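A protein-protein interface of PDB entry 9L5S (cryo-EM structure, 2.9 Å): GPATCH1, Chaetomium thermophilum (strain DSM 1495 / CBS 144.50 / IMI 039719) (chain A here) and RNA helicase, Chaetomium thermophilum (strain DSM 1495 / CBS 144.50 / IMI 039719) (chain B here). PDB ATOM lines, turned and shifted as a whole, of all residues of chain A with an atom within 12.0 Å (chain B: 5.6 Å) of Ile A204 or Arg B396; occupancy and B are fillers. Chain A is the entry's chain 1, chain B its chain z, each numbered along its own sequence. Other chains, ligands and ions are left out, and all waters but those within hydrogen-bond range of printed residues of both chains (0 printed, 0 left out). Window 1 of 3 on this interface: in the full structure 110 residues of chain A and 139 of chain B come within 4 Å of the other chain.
NH1 of Arg B396 lies within hydrogen-bond range of O of Arg B338. The side-chain carboxylate of Glu B393 is in salt-bridge range of the guanidinium group of Arg B396 (2.6 Å). The side-chain amide oxygen (OE1) of Gln B427 lies close to the backbone carbonyl oxygen (O) of Gln B395. The backbone NH (N) of Ser B397 lies close to the side-chain amide nitrogen (NE2) of Gln B427, at 3.2 Å.
Gln B395 touches Val A201 (NE2 to CG1, 3.97 Å). Met A203 touches Gln B427 (CE to N, 3.4 Å). Ile A204 touches Val B391 (CD1 to CG1, 3.7 Å). Ile A204 touches Arg B396 (CD1 to CB, 3.7 Å). Phe A206 touches Ala B339.
Ile A171 touches none of the printed residues of chain B. Asn A200 touches none of the printed residues of chain B. Of the printed residues of chain B, Val A201 touches Gln B395 (3.97 Å). Ile A204 touches just these residues of chain B: Val B391 and Arg B396. No residue of chain A comes within 4 Å of Leu B337. No residue of chain A comes within 4 Å of Thr B390. Val B391 touches just one residue of chain A: Ile A204 (3.7 Å). No residue of chain A comes within 4 Å of Ser B397. Of the printed residues of chain A, Gln B427 touches Met A203 (3.4 Å). The nearest residue of chain A that does not touch Arg B396 is Phe A206 (4.8 Å). The nearest printed residue of chain B that does not touch Met A203 is Gln B395 (4.7 Å).
Of the 15 printed residues of chain B, 5 touch a printed residue of chain A. Hydrophobic or aromatic side chains of chain B within 4 Å of the printed part of chain A: Ala B339 and Val B391. Of the 10 printed residues of chain A, 4 touch a printed residue of chain B. Printed residues of chain A that touch a printed residue of chain B: Val A201, Met A203, Ile A204 and Phe A206. Hydrophobic or aromatic side chains of chain A that line the printed part of chain B: Val A201, Met A203, Ile A204 and Phe A206. Among the printed residues, no Asp or Glu carboxylate lies within 4 Å of a Lys or Arg side-chain nitrogen of the other chain.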
ATOM      1  N   ILE A 171      13.906 -34.352 -22.102  1.00  0.00           N
ATOM      2  CA  ILE A 171      13.297 -35.548 -22.669  1.00  0.00           C
ATOM      3  C   ILE A 171      14.234 -36.127 -23.722  1.00  0.00           C
ATOM      4  O   ILE A 171      15.234 -35.519 -24.104  1.00  0.00           O
ATOM      5  CB  ILE A 171      11.907 -35.280 -23.290  1.00  0.00           C
ATOM      6  CG1 ILE A 171      12.048 -34.541 -24.619  1.00  0.00           C
ATOM      7  CG2 ILE A 171      11.007 -34.511 -22.328  1.00  0.00           C
ATOM      8  CD1 ILE A 171      10.845 -34.691 -25.505  1.00  0.00           C
ATOM      9  N   ASN A 200      17.874 -30.726 -19.718  1.00  0.00           N
ATOM     10  CA  ASN A 200      16.868 -29.787 -20.199  1.00  0.00           C
ATOM     11  C   ASN A 200      17.556 -28.654 -20.952  1.00  0.00           C
ATOM     12  O   ASN A 200      18.254 -27.832 -20.351  1.00  0.00           O
ATOM     13  CB  ASN A 200      16.042 -29.243 -19.035  1.00  0.00           C
ATOM     14  CG  ASN A 200      14.764 -28.566 -19.493  1.00  0.00           C
ATOM     15  OD1 ASN A 200      14.450 -28.542 -20.682  1.00  0.00           O
ATOM     16  ND2 ASN A 200      14.020 -28.010 -18.545  1.00  0.00           N
ATOM     17  N   VAL A 201      17.365 -28.618 -22.265  1.00  0.00           N
ATOM     18  CA  VAL A 201      17.758 -27.440 -23.045  1.00  0.00           C
ATOM     19  C   VAL A 201      16.839 -26.276 -22.674  1.00  0.00           C
ATOM     20  O   VAL A 201      15.634 -26.488 -22.453  1.00  0.00           O
ATOM     21  CB  VAL A 201      17.721 -27.764 -24.554  1.00  0.00           C
ATOM     22  CG1 VAL A 201      16.320 -28.136 -25.038  1.00  0.00           C
ATOM     23  CG2 VAL A 201      18.287 -26.624 -25.389  1.00  0.00           C
ATOM     24  N   PRO A 202      17.358 -25.066 -22.477  1.00  0.00           N
ATOM     25  CA  PRO A 202      16.489 -23.952 -22.080  1.00  0.00           C
ATOM     26  C   PRO A 202      15.631 -23.445 -23.230  1.00  0.00           C
ATOM     27  O   PRO A 202      15.940 -23.629 -24.410  1.00  0.00           O
ATOM     28  CB  PRO A 202      17.480 -22.878 -21.612  1.00  0.00           C
ATOM     29  CG  PRO A 202      18.764 -23.226 -22.291  1.00  0.00           C
ATOM     30  CD  PRO A 202      18.786 -24.721 -22.354  1.00  0.00           C
ATOM     31  N   MET A 203      14.531 -22.789 -22.858  1.00  0.00           N
ATOM     32  CA  MET A 203      13.701 -22.089 -23.826  1.00  0.00           C
ATOM     33  C   MET A 203      14.373 -20.819 -24.327  1.00  0.00           C
ATOM     34  O   MET A 203      15.429 -20.391 -23.851  1.00  0.00           O
ATOM     35  CB  MET A 203      12.328 -21.741 -23.243  1.00  0.00           C
ATOM     36  CG  MET A 203      11.675 -22.842 -22.459  1.00  0.00           C
ATOM     37  SD  MET A 203      10.925 -23.926 -23.695  1.00  0.00           S
ATOM     38  CE  MET A 203       9.896 -24.975 -22.681  1.00  0.00           C
ATOM     39  N   ILE A 204      13.727 -20.227 -25.323  1.00  0.00           N
ATOM     40  CA  ILE A 204      14.148 -18.986 -25.950  1.00  0.00           C
ATOM     41  C   ILE A 204      13.155 -17.897 -25.576  1.00  0.00           C
ATOM     42  O   ILE A 204      11.951 -18.157 -25.447  1.00  0.00           O
ATOM     43  CB  ILE A 204      14.245 -19.158 -27.477  1.00  0.00           C
ATOM     44  CG1 ILE A 204      12.997 -19.882 -27.987  1.00  0.00           C
ATOM     45  CG2 ILE A 204      15.507 -19.911 -27.843  1.00  0.00           C
ATOM     46  CD1 ILE A 204      12.706 -19.671 -29.432  1.00  0.00           C
ATOM     47  N   SER A 205      13.662 -16.684 -25.378  1.00  0.00           N
ATOM     48  CA  SER A 205      12.824 -15.534 -25.045  1.00  0.00           C
ATOM     49  C   SER A 205      13.365 -14.348 -25.834  1.00  0.00           C
ATOM     50  O   SER A 205      14.312 -13.687 -25.398  1.00  0.00           O
ATOM     51  CB  SER A 205      12.830 -15.260 -23.546  1.00  0.00           C
ATOM     52  OG  SER A 205      12.316 -16.366 -22.823  1.00  0.00           O
ATOM     53  N   PHE A 206      12.771 -14.089 -26.996  1.00  0.00           N
ATOM     54  CA  PHE A 206      13.219 -12.990 -27.837  1.00  0.00           C
ATOM     55  C   PHE A 206      12.842 -11.652 -27.218  1.00  0.00           C
ATOM     56  O   PHE A 206      11.721 -11.466 -26.733  1.00  0.00           O
ATOM     57  CB  PHE A 206      12.626 -13.095 -29.242  1.00  0.00           C
ATOM     58  CG  PHE A 206      12.919 -14.394 -29.931  1.00  0.00           C
ATOM     59  CD1 PHE A 206      14.223 -14.759 -30.217  1.00  0.00           C
ATOM     60  CD2 PHE A 206      11.890 -15.233 -30.330  1.00  0.00           C
ATOM     61  CE1 PHE A 206      14.498 -15.948 -30.857  1.00  0.00           C
ATOM     62  CE2 PHE A 206      12.160 -16.420 -30.980  1.00  0.00           C
ATOM     63  CZ  PHE A 206      13.468 -16.772 -31.248  1.00  0.00           C
ATOM     64  N   VAL A 207      13.797 -10.722 -27.228  1.00  0.00           N
ATOM     65  CA  VAL A 207      13.530  -9.362 -26.784  1.00  0.00           C
ATOM     66  C   VAL A 207      12.588  -8.693 -27.777  1.00  0.00           C
ATOM     67  O   VAL A 207      12.707  -8.883 -28.995  1.00  0.00           O
ATOM     68  CB  VAL A 207      14.846  -8.580 -26.636  1.00  0.00           C
ATOM     69  CG1 VAL A 207      14.615  -7.256 -25.922  1.00  0.00           C
ATOM     70  CG2 VAL A 207      15.876  -9.418 -25.895  1.00  0.00           C
ATOM     71  N   ARG A 208      11.624  -7.935 -27.253  1.00  0.00           N
ATOM     72  CA  ARG A 208      10.638  -7.270 -28.094  1.00  0.00           C
ATOM     73  C   ARG A 208      11.304  -6.244 -29.003  1.00  0.00           C
ATOM     74  O   ARG A 208      12.131  -5.444 -28.558  1.00  0.00           O
ATOM     75  CB  ARG A 208       9.578  -6.600 -27.219  1.00  0.00           C
ATOM     76  CG  ARG A 208       8.505  -5.864 -27.995  1.00  0.00           C
ATOM     77  CD  ARG A 208       7.337  -5.483 -27.103  1.00  0.00           C
ATOM     78  NE  ARG A 208       6.389  -6.582 -26.960  1.00  0.00           N
ATOM     79  CZ  ARG A 208       5.154  -6.451 -26.499  1.00  0.00           C
ATOM     80  NH1 ARG A 208       4.677  -5.276 -26.123  1.00  0.00           N
ATOM     81  NH2 ARG A 208       4.376  -7.526 -26.413  1.00  0.00           N
ATOM     82  N   LEU B 337      10.186 -14.464 -36.541  1.00  0.00           N
ATOM     83  CA  LEU B 337      10.109 -15.853 -36.120  1.00  0.00           C
ATOM     84  C   LEU B 337       8.965 -16.013 -35.131  1.00  0.00           C
ATOM     85  O   LEU B 337       8.676 -15.110 -34.340  1.00  0.00           O
ATOM     86  CB  LEU B 337      11.423 -16.323 -35.481  1.00  0.00           C
ATOM     87  CG  LEU B 337      12.516 -16.818 -36.430  1.00  0.00           C
ATOM     88  CD1 LEU B 337      13.706 -17.350 -35.643  1.00  0.00           C
ATOM     89  CD2 LEU B 337      11.972 -17.883 -37.368  1.00  0.00           C
ATOM     90  N   ARG B 338       8.323 -17.177 -35.184  1.00  0.00           N
ATOM     91  CA  ARG B 338       7.215 -17.515 -34.301  1.00  0.00           C
ATOM     92  C   ARG B 338       7.720 -18.408 -33.176  1.00  0.00           C
ATOM     93  O   ARG B 338       8.413 -19.399 -33.427  1.00  0.00           O
ATOM     94  CB  ARG B 338       6.099 -18.222 -35.072  1.00  0.00           C
ATOM     95  CG  ARG B 338       4.877 -18.533 -34.228  1.00  0.00           C
ATOM     96  CD  ARG B 338       3.756 -19.158 -35.045  1.00  0.00           C
ATOM     97  NE  ARG B 338       3.124 -18.203 -35.947  1.00  0.00           N
ATOM     98  CZ  ARG B 338       3.060 -18.347 -37.263  1.00  0.00           C
ATOM     99  NH1 ARG B 338       3.578 -19.403 -37.869  1.00  0.00           N
ATOM    100  NH2 ARG B 338       2.460 -17.409 -37.991  1.00  0.00           N
ATOM    101  N   ALA B 339       7.374 -18.054 -31.940  1.00  0.00           N
ATOM    102  CA  ALA B 339       7.811 -18.804 -30.765  1.00  0.00           C
ATOM    103  C   ALA B 339       6.642 -18.907 -29.796  1.00  0.00           C
ATOM    104  O   ALA B 339       6.221 -17.900 -29.218  1.00  0.00           O
ATOM    105  CB  ALA B 339       9.014 -18.137 -30.098  1.00  0.00           C
ATOM    106  N   TYR B 340       6.117 -20.118 -29.622  1.00  0.00           N
ATOM    107  CA  TYR B 340       5.026 -20.352 -28.684  1.00  0.00           C
ATOM    108  C   TYR B 340       5.576 -20.345 -27.264  1.00  0.00           C
ATOM    109  O   TYR B 340       6.441 -21.161 -26.923  1.00  0.00           O
ATOM    110  CB  TYR B 340       4.327 -21.675 -29.000  1.00  0.00           C
ATOM    111  CG  TYR B 340       3.291 -22.108 -27.980  1.00  0.00           C
ATOM    112  CD1 TYR B 340       1.991 -21.624 -28.037  1.00  0.00           C
ATOM    113  CD2 TYR B 340       3.605 -23.026 -26.980  1.00  0.00           C
ATOM    114  CE1 TYR B 340       1.037 -22.019 -27.116  1.00  0.00           C
ATOM    115  CE2 TYR B 340       2.658 -23.426 -26.054  1.00  0.00           C
ATOM    116  CZ  TYR B 340       1.377 -22.920 -26.127  1.00  0.00           C
ATOM    117  OH  TYR B 340       0.430 -23.318 -25.211  1.00  0.00           O
ATOM    118  N   GLU B 347       1.551 -17.188 -29.003  1.00  0.00           N
ATOM    119  CA  GLU B 347       2.629 -17.101 -29.972  1.00  0.00           C
ATOM    120  C   GLU B 347       3.296 -15.732 -29.888  1.00  0.00           C
ATOM    121  O   GLU B 347       2.781 -14.800 -29.267  1.00  0.00           O
ATOM    122  CB  GLU B 347       2.105 -17.350 -31.388  1.00  0.00           C
ATOM    123  CG  GLU B 347       1.294 -18.631 -31.545  1.00  0.00           C
ATOM    124  CD  GLU B 347       2.132 -19.895 -31.440  1.00  0.00           C
ATOM    125  OE1 GLU B 347       3.366 -19.822 -31.622  1.00  0.00           O
ATOM    126  OE2 GLU B 347       1.551 -20.968 -31.179  1.00  0.00           O
ATOM    127  N   THR B 390      19.804 -21.532 -36.909  1.00  0.00           N
ATOM    128  CA  THR B 390      18.547 -21.040 -36.370  1.00  0.00           C
ATOM    129  C   THR B 390      18.113 -21.875 -35.168  1.00  0.00           C
ATOM    130  O   THR B 390      18.609 -22.980 -34.929  1.00  0.00           O
ATOM    131  CB  THR B 390      17.453 -21.062 -37.439  1.00  0.00           C
ATOM    132  OG1 THR B 390      17.156 -22.417 -37.793  1.00  0.00           O
ATOM    133  CG2 THR B 390      17.904 -20.307 -38.678  1.00  0.00           C
ATOM    134  N   VAL B 391      17.186 -21.312 -34.396  1.00  0.00           N
ATOM    135  CA  VAL B 391      16.597 -22.041 -33.268  1.00  0.00           C
ATOM    136  C   VAL B 391      15.816 -23.232 -33.810  1.00  0.00           C
ATOM    137  O   VAL B 391      15.168 -23.108 -34.870  1.00  0.00           O
ATOM    138  CB  VAL B 391      15.694 -21.102 -32.445  1.00  0.00           C
ATOM    139  CG1 VAL B 391      14.801 -21.873 -31.485  1.00  0.00           C
ATOM    140  CG2 VAL B 391      16.540 -20.089 -31.687  1.00  0.00           C
ATOM    141  N   PRO B 392      15.901 -24.414 -33.188  1.00  0.00           N
ATOM    142  CA  PRO B 392      15.115 -25.563 -33.660  1.00  0.00           C
ATOM    143  C   PRO B 392      13.619 -25.280 -33.661  1.00  0.00           C
ATOM    144  O   PRO B 392      13.072 -24.707 -32.716  1.00  0.00           O
ATOM    145  CB  PRO B 392      15.473 -26.668 -32.661  1.00  0.00           C
ATOM    146  CG  PRO B 392      16.829 -26.301 -32.173  1.00  0.00           C
ATOM    147  CD  PRO B 392      16.878 -24.800 -32.154  1.00  0.00           C
ATOM    148  N   GLU B 393      12.963 -25.687 -34.751  1.00  0.00           N
ATOM    149  CA  GLU B 393      11.537 -25.427 -34.914  1.00  0.00           C
ATOM    150  C   GLU B 393      10.699 -26.248 -33.943  1.00  0.00           C
ATOM    151  O   GLU B 393       9.576 -25.854 -33.609  1.00  0.00           O
ATOM    152  CB  GLU B 393      11.116 -25.720 -36.353  1.00  0.00           C
ATOM    153  CG  GLU B 393      11.502 -24.662 -37.372  1.00  0.00           C
ATOM    154  CD  GLU B 393      10.506 -23.526 -37.434  1.00  0.00           C
ATOM    155  OE1 GLU B 393       9.375 -23.705 -36.938  1.00  0.00           O
ATOM    156  OE2 GLU B 393      10.852 -22.462 -37.986  1.00  0.00           O
ATOM    157  N   ILE B 394      11.224 -27.385 -33.479  1.00  0.00           N
ATOM    158  CA  ILE B 394      10.503 -28.195 -32.509  1.00  0.00           C
ATOM    159  C   ILE B 394      10.568 -27.583 -31.115  1.00  0.00           C
ATOM    160  O   ILE B 394       9.813 -27.990 -30.225  1.00  0.00           O
ATOM    161  CB  ILE B 394      11.048 -29.639 -32.524  1.00  0.00           C
ATOM    162  CG1 ILE B 394       9.962 -30.638 -32.113  1.00  0.00           C
ATOM    163  CG2 ILE B 394      12.280 -29.769 -31.637  1.00  0.00           C
ATOM    164  CD1 ILE B 394      10.331 -32.082 -32.382  1.00  0.00           C
ATOM    165  N   GLN B 395      11.442 -26.599 -30.904  1.00  0.00           N
ATOM    166  CA  GLN B 395      11.583 -25.955 -29.607  1.00  0.00           C
ATOM    167  C   GLN B 395      10.742 -24.691 -29.467  1.00  0.00           C
ATOM    168  O   GLN B 395      10.661 -24.143 -28.363  1.00  0.00           O
ATOM    169  CB  GLN B 395      13.054 -25.611 -29.349  1.00  0.00           C
ATOM    170  CG  GLN B 395      13.950 -26.819 -29.147  1.00  0.00           C
ATOM    171  CD  GLN B 395      15.330 -26.442 -28.647  1.00  0.00           C
ATOM    172  OE1 GLN B 395      15.512 -25.392 -28.031  1.00  0.00           O
ATOM    173  NE2 GLN B 395      16.311 -27.295 -28.914  1.00  0.00           N
ATOM    174  N   ARG B 396      10.117 -24.218 -30.543  1.00  0.00           N
ATOM    175  CA  ARG B 396       9.342 -22.978 -30.513  1.00  0.00           C
ATOM    176  C   ARG B 396       8.028 -23.152 -31.268  1.00  0.00           C
ATOM    177  O   ARG B 396       7.624 -22.309 -32.070  1.00  0.00           O
ATOM    178  CB  ARG B 396      10.157 -21.812 -31.072  1.00  0.00           C
ATOM    179  CG  ARG B 396      10.891 -22.107 -32.369  1.00  0.00           C
ATOM    180  CD  ARG B 396      11.523 -20.840 -32.921  1.00  0.00           C
ATOM    181  NE  ARG B 396      12.261 -21.079 -34.154  1.00  0.00           N
ATOM    182  CZ  ARG B 396      11.744 -20.971 -35.369  1.00  0.00           C
ATOM    183  NH1 ARG B 396      10.476 -20.642 -35.554  1.00  0.00           N
ATOM    184  NH2 ARG B 396      12.518 -21.199 -36.427  1.00  0.00           N
ATOM    185  N   SER B 397       7.341 -24.261 -31.010  1.00  0.00           N
ATOM    186  CA  SER B 397       6.059 -24.539 -31.640  1.00  0.00           C
ATOM    187  C   SER B 397       5.145 -25.224 -30.635  1.00  0.00           C
ATOM    188  O   SER B 397       5.589 -25.712 -29.594  1.00  0.00           O
ATOM    189  CB  SER B 397       6.223 -25.411 -32.892  1.00  0.00           C
ATOM    190  OG  SER B 397       6.670 -26.711 -32.550  1.00  0.00           O
ATOM    191  N   ASN B 398       3.853 -25.240 -30.950  1.00  0.00           N
ATOM    192  CA  ASN B 398       2.873 -25.927 -30.115  1.00  0.00           C
ATOM    193  C   ASN B 398       2.973 -27.428 -30.357  1.00  0.00           C
ATOM    194  O   ASN B 398       2.583 -27.916 -31.419  1.00  0.00           O
ATOM    195  CB  ASN B 398       1.468 -25.417 -30.420  1.00  0.00           C
ATOM    196  CG  ASN B 398       0.561 -25.446 -29.207  1.00  0.00           C
ATOM    197  OD1 ASN B 398       1.024 -25.370 -28.070  1.00  0.00           O
ATOM    198  ND2 ASN B 398      -0.740 -25.558 -29.445  1.00  0.00           N
ATOM    199  N   GLN B 427       7.552 -27.472 -22.396  1.00  0.00           N
ATOM    200  CA  GLN B 427       6.659 -27.133 -23.498  1.00  0.00           C
ATOM    201  C   GLN B 427       5.672 -28.263 -23.770  1.00  0.00           C
ATOM    202  O   GLN B 427       4.471 -28.021 -23.958  1.00  0.00           O
ATOM    203  CB  GLN B 427       7.472 -26.817 -24.752  1.00  0.00           C
ATOM    204  CG  GLN B 427       6.674 -26.171 -25.870  1.00  0.00           C
ATOM    205  CD  GLN B 427       7.559 -25.672 -26.998  1.00  0.00           C
ATOM    206  OE1 GLN B 427       8.741 -26.007 -27.068  1.00  0.00           O
ATOM    207  NE2 GLN B 427       6.991 -24.862 -27.885  1.00  0.00           N
